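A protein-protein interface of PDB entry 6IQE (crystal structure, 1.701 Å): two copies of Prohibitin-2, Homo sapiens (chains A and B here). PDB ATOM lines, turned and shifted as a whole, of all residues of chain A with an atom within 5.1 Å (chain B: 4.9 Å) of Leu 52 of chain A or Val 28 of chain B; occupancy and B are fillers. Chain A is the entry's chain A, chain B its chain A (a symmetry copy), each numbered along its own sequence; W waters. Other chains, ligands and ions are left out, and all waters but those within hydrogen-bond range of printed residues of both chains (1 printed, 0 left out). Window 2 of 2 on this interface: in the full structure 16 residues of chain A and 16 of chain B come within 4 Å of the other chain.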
ATOM      1  N   GLU A  47      14.427  -1.371 -19.980  1.00  0.00           N
ATOM      2  CA  GLU A  47      15.604  -1.001 -20.767  1.00  0.00           C
ATOM      3  C   GLU A  47      15.614  -1.730 -22.124  1.00  0.00           C
ATOM      4  O   GLU A  47      15.944  -1.139 -23.153  1.00  0.00           O
ATOM      5  CB  GLU A  47      16.887  -1.302 -19.985  1.00  0.00           C
ATOM      6  CG  GLU A  47      18.198  -1.063 -20.778  1.00  0.00           C
ATOM      7  CD  GLU A  47      18.434   0.405 -21.127  1.00  0.00           C
ATOM      8  OE1 GLU A  47      17.785   1.290 -20.530  1.00  0.00           O
ATOM      9  OE2 GLU A  47      19.273   0.681 -22.006  1.00  0.00           O
ATOM     10  N   ALA A  48      15.256  -3.009 -22.117  1.00  0.00           N
ATOM     11  CA  ALA A  48      15.148  -3.778 -23.363  1.00  0.00           C
ATOM     12  C   ALA A  48      14.179  -3.132 -24.336  1.00  0.00           C
ATOM     13  O   ALA A  48      14.483  -3.001 -25.526  1.00  0.00           O
ATOM     14  CB  ALA A  48      14.740  -5.222 -23.065  1.00  0.00           C
ATOM     15  N   ALA A  49      13.040  -2.687 -23.806  1.00  0.00           N
ATOM     16  CA  ALA A  49      11.987  -2.011 -24.589  1.00  0.00           C
ATOM     17  C   ALA A  49      12.438  -0.626 -25.081  1.00  0.00           C
ATOM     18  O   ALA A  49      12.202  -0.268 -26.244  1.00  0.00           O
ATOM     19  CB  ALA A  49      10.694  -1.884 -23.767  1.00  0.00           C
ATOM     20  N   LYS A  50      13.106   0.126 -24.216  1.00  0.00           N
ATOM     21  CA  LYS A  50      13.712   1.395 -24.614  1.00  0.00           C
ATOM     22  C   LYS A  50      14.654   1.207 -25.805  1.00  0.00           C
ATOM     23  O   LYS A  50      14.571   1.927 -26.802  1.00  0.00           O
ATOM     24  CB  LYS A  50      14.461   2.029 -23.438  1.00  0.00           C
ATOM     25  CG  LYS A  50      15.001   3.431 -23.738  1.00  0.00           C
ATOM     26  CD  LYS A  50      15.815   3.961 -22.565  1.00  0.00           C
ATOM     27  CE  LYS A  50      16.661   5.167 -22.967  1.00  0.00           C
ATOM     28  NZ  LYS A  50      17.705   5.473 -21.938  1.00  0.00           N
ATOM     29  N   MET A  51      15.539   0.217 -25.724  1.00  0.00           N
ATOM     30  CA  MET A  51      16.462  -0.025 -26.817  1.00  0.00           C
ATOM     31  C   MET A  51      15.763  -0.420 -28.119  1.00  0.00           C
ATOM     32  O   MET A  51      16.188  -0.019 -29.206  1.00  0.00           O
ATOM     33  CB  MET A  51      17.452  -1.108 -26.421  1.00  0.00           C
ATOM     34  CG  MET A  51      18.345  -0.711 -25.254  1.00  0.00           C
ATOM     35  SD  MET A  51      19.379  -2.090 -24.701  1.00  0.00           S
ATOM     36  CE  MET A  51      20.469  -2.287 -26.114  1.00  0.00           C
ATOM     37  N   LEU A  52      14.703  -1.215 -28.020  1.00  0.00           N
ATOM     38  CA  LEU A  52      13.985  -1.627 -29.207  1.00  0.00           C
ATOM     39  C   LEU A  52      13.305  -0.403 -29.826  1.00  0.00           C
ATOM     40  O   LEU A  52      13.311  -0.222 -31.047  1.00  0.00           O
ATOM     41  CB  LEU A  52      12.980  -2.729 -28.871  1.00  0.00           C
ATOM     42  CG  LEU A  52      12.092  -3.186 -30.040  1.00  0.00           C
ATOM     43  CD1 LEU A  52      12.926  -3.716 -31.210  1.00  0.00           C
ATOM     44  CD2 LEU A  52      11.058  -4.220 -29.566  1.00  0.00           C
ATOM     45  N   GLY A  53      12.746   0.453 -28.985  1.00  0.00           N
ATOM     46  CA  GLY A  53      12.124   1.672 -29.479  1.00  0.00           C
ATOM     47  C   GLY A  53      13.110   2.569 -30.217  1.00  0.00           C
ATOM     48  O   GLY A  53      12.766   3.205 -31.223  1.00  0.00           O
ATOM     49  N   GLU A  54      14.345   2.617 -29.724  1.00  0.00           N
ATOM     50  CA  GLU A  54      15.379   3.443 -30.354  1.00  0.00           C
ATOM     51  C   GLU A  54      15.797   2.856 -31.695  1.00  0.00           C
ATOM     52  O   GLU A  54      16.055   3.590 -32.654  1.00  0.00           O
ATOM     53  CB  GLU A  54      16.586   3.601 -29.421  1.00  0.00           C
ATOM     54  CG  GLU A  54      16.331   4.609 -28.296  1.00  0.00           C
ATOM     55  CD  GLU A  54      17.372   4.573 -27.180  1.00  0.00           C
ATOM     56  OE1 GLU A  54      18.266   3.694 -27.206  1.00  0.00           O
ATOM     57  OE2 GLU A  54      17.284   5.428 -26.267  1.00  0.00           O
ATOM     58  N   ALA A  55      15.851   1.530 -31.769  1.00  0.00           N
ATOM     59  CA  ALA A  55      16.166   0.847 -33.022  1.00  0.00           C
ATOM     60  C   ALA A  55      15.047   0.988 -34.052  1.00  0.00           C
ATOM     61  O   ALA A  55      15.293   0.888 -35.253  1.00  0.00           O
ATOM     62  CB  ALA A  55      16.462  -0.626 -32.766  1.00  0.00           C
ATOM     63  N   LEU A  56      13.820   1.202 -33.584  1.00  0.00           N
ATOM     64  CA  LEU A  56      12.703   1.467 -34.480  1.00  0.00           C
ATOM     65  C   LEU A  56      12.777   2.884 -35.039  1.00  0.00           C
ATOM     66  O   LEU A  56      12.452   3.111 -36.205  1.00  0.00           O
ATOM     67  CB  LEU A  56      11.364   1.273 -33.765  1.00  0.00           C
ATOM     68  CG  LEU A  56      10.953  -0.129 -33.319  1.00  0.00           C
ATOM     69  CD1 LEU A  56       9.637  -0.080 -32.563  1.00  0.00           C
ATOM     70  CD2 LEU A  56      10.804  -1.003 -34.526  1.00  0.00           C
ATOM     71  N   ALA B  24       4.433  -1.419 -34.410  1.00  0.00           N
ATOM     72  CA  ALA B  24       5.631  -1.731 -33.642  1.00  0.00           C
ATOM     73  C   ALA B  24       5.898  -0.655 -32.595  1.00  0.00           C
ATOM     74  O   ALA B  24       6.154  -0.960 -31.429  1.00  0.00           O
ATOM     75  CB  ALA B  24       6.844  -1.887 -34.569  1.00  0.00           C
ATOM     76  N   GLN B  25       5.826   0.609 -32.993  1.00  0.00           N
ATOM     77  CA  GLN B  25       6.099   1.681 -32.044  1.00  0.00           C
ATOM     78  C   GLN B  25       5.044   1.708 -30.933  1.00  0.00           C
ATOM     79  O   GLN B  25       5.369   1.961 -29.766  1.00  0.00           O
ATOM     80  CB  GLN B  25       6.180   3.039 -32.745  1.00  0.00           C
ATOM     81  CG  GLN B  25       6.743   4.128 -31.827  1.00  0.00           C
ATOM     82  CD  GLN B  25       8.204   3.876 -31.428  1.00  0.00           C
ATOM     83  OE1 GLN B  25       9.080   3.710 -32.280  1.00  0.00           O
ATOM     84  NE2 GLN B  25       8.462   3.837 -30.120  1.00  0.00           N
ATOM     85  N   PHE B  26       3.792   1.444 -31.295  1.00  0.00           N
ATOM     86  CA  PHE B  26       2.708   1.387 -30.320  1.00  0.00           C
ATOM     87  C   PHE B  26       2.943   0.299 -29.267  1.00  0.00           C
ATOM     88  O   PHE B  26       2.747   0.537 -28.077  1.00  0.00           O
ATOM     89  CB  PHE B  26       1.360   1.160 -31.015  1.00  0.00           C
ATOM     90  CG  PHE B  26       0.198   1.039 -30.065  1.00  0.00           C
ATOM     91  CD1 PHE B  26      -0.482   2.168 -29.632  1.00  0.00           C
ATOM     92  CD2 PHE B  26      -0.216  -0.200 -29.611  1.00  0.00           C
ATOM     93  CE1 PHE B  26      -1.552   2.056 -28.754  1.00  0.00           C
ATOM     94  CE2 PHE B  26      -1.280  -0.317 -28.730  1.00  0.00           C
ATOM     95  CZ  PHE B  26      -1.948   0.813 -28.304  1.00  0.00           C
ATOM     96  N   LEU B  27       3.369  -0.884 -29.705  1.00  0.00           N
ATOM     97  CA  LEU B  27       3.575  -2.026 -28.817  1.00  0.00           C
ATOM     98  C   LEU B  27       4.762  -1.800 -27.897  1.00  0.00           C
ATOM     99  O   LEU B  27       4.723  -2.160 -26.717  1.00  0.00           O
ATOM    100  CB  LEU B  27       3.794  -3.306 -29.628  1.00  0.00           C
ATOM    101  CG  LEU B  27       2.479  -3.816 -30.218  1.00  0.00           C
ATOM    102  CD1 LEU B  27       2.753  -4.818 -31.295  1.00  0.00           C
ATOM    103  CD2 LEU B  27       1.587  -4.422 -29.147  1.00  0.00           C
ATOM    104  N   VAL B  28       5.811  -1.197 -28.441  1.00  0.00           N
ATOM    105  CA  VAL B  28       6.968  -0.813 -27.629  1.00  0.00           C
ATOM    106  C   VAL B  28       6.588   0.172 -26.526  1.00  0.00           C
ATOM    107  O   VAL B  28       6.954  -0.001 -25.350  1.00  0.00           O
ATOM    108  CB  VAL B  28       8.070  -0.191 -28.501  1.00  0.00           C
ATOM    109  CG1 VAL B  28       9.002   0.688 -27.665  1.00  0.00           C
ATOM    110  CG2 VAL B  28       8.836  -1.300 -29.198  1.00  0.00           C
ATOM    111  N   GLU B  29       5.846   1.199 -26.907  1.00  0.00           N
ATOM    112  CA  GLU B  29       5.448   2.221 -25.947  1.00  0.00           C
ATOM    113  C   GLU B  29       4.535   1.618 -24.869  1.00  0.00           C
ATOM    114  O   GLU B  29       4.617   1.987 -23.691  1.00  0.00           O
ATOM    115  CB  GLU B  29       4.755   3.386 -26.651  1.00  0.00           C
ATOM    116  CG  GLU B  29       4.568   4.596 -25.752  1.00  0.00           C
ATOM    117  CD  GLU B  29       5.885   5.082 -25.153  1.00  0.00           C
ATOM    118  OE1 GLU B  29       6.901   5.122 -25.887  1.00  0.00           O
ATOM    119  OE2 GLU B  29       5.903   5.408 -23.944  1.00  0.00           O
ATOM    120  N   LYS B  30       3.670   0.695 -25.279  1.00  0.00           N
ATOM    121  CA  LYS B  30       2.779   0.007 -24.346  1.00  0.00           C
ATOM    122  C   LYS B  30       3.590  -0.795 -23.316  1.00  0.00           C
ATOM    123  O   LYS B  30       3.327  -0.722 -22.118  1.00  0.00           O
ATOM    124  CB  LYS B  30       1.814  -0.902 -25.108  1.00  0.00           C
ATOM    125  CG  LYS B  30       0.849  -1.711 -24.247  1.00  0.00           C
ATOM    126  CD  LYS B  30      -0.232  -2.327 -25.125  1.00  0.00           C
ATOM    127  CE  LYS B  30      -0.803  -3.601 -24.544  1.00  0.00           C
ATOM    128  NZ  LYS B  30      -1.451  -3.382 -23.241  1.00  0.00           N
ATOM    129  N   ALA B  31       4.587  -1.536 -23.790  1.00  0.00           N
ATOM    130  CA  ALA B  31       5.434  -2.357 -22.916  1.00  0.00           C
ATOM    131  C   ALA B  31       6.260  -1.482 -21.981  1.00  0.00           C
ATOM    132  O   ALA B  31       6.396  -1.788 -20.788  1.00  0.00           O
ATOM    133  CB  ALA B  31       6.345  -3.262 -23.745  1.00  0.00           C
ATOM    134  N   LYS B  32       6.798  -0.389 -22.518  1.00  0.00           N
ATOM    135  CA  LYS B  32       7.562   0.576 -21.731  1.00  0.00           C
ATOM    136  C   LYS B  32       6.742   1.102 -20.563  1.00  0.00           C
ATOM    137  O   LYS B  32       7.189   1.139 -19.420  1.00  0.00           O
ATOM    138  CB  LYS B  32       8.001   1.761 -22.594  1.00  0.00           C
ATOM    139  CG  LYS B  32       9.282   1.566 -23.363  1.00  0.00           C
ATOM    140  CD  LYS B  32       9.907   2.929 -23.652  1.00  0.00           C
ATOM    141  CE  LYS B  32      10.163   3.133 -25.119  1.00  0.00           C
ATOM    142  NZ  LYS B  32      10.880   4.422 -25.323  1.00  0.00           N
HETATM  143  O   HOH W   1      12.924   4.103 -26.772  1.00  0.00           O
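No position is printed for both chains. Of the 9 pairs that touch across the chains among the printed residues, none has its exchanged pair printed and touching as well.
Printed residues of chain B that touch a printed residue of chain A: Ala 24, Gln 25, Val 28 and Lys 32. Along chain A the printed residues that touch a printed residue of chain B span positions 49 to 56. Among the printed residues, 9 pairs touch across the chains. Among the printed residues, no Asp or Glu carboxylate lies within 4 Å of a Lys or Arg side-chain nitrogen of the other chain.
Ala 49 of chain A touches Val 28 of chain B. CG of Lys 32 of chain B touches CB of Ala 49 of chain A, at 3.7 Å. Lys 50 of chain A touches Lys 32 of chain B. Leu 52 of chain A touches Val 28 of chain B (CD2 to CG2, 3.7 Å). Gln 25 of chain B touches Gly 53 of chain A. Gly 53 of chain A touches Val 28 of chain B. CD1 of Leu 56 of chain A touches O of Ala 24 of chain B, 3.8 Å away. Leu 56 of chain A touches Gln 25 of chain B. CG2 of Val 28 of chain B touches CD1 of Leu 56 of chain A, at 3.7 Å.
Water W1 bridges NZ of Lys 32 of chain B (2.5 Å) and O of Lys 50 of chain A (2.7 Å).
Printed residues of chain B within 4 Å of Ala 49 of chain A: Val 28 (3.6 Å) and Lys 32 (3.7 Å). Of chain B, only Val 28 comes within 4 Å of Leu 52 of chain A. Of the printed residues of chain A, Ala 24 of chain B touches Leu 56. Val 28 of chain B touches just these residues of chain A: Ala 49 (3.6 Å), Leu 52 (3.7 Å), Gly 53 (3.7 Å) and Leu 56 (3.7 Å). The nearest printed residue of chain B that does not touch Leu 52 of chain A is Gln 25 of chain B (5.9 Å). The nearest printed residue of chain A that does not touch Val 28 of chain B is Lys 50 of chain A (5.4 Å).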
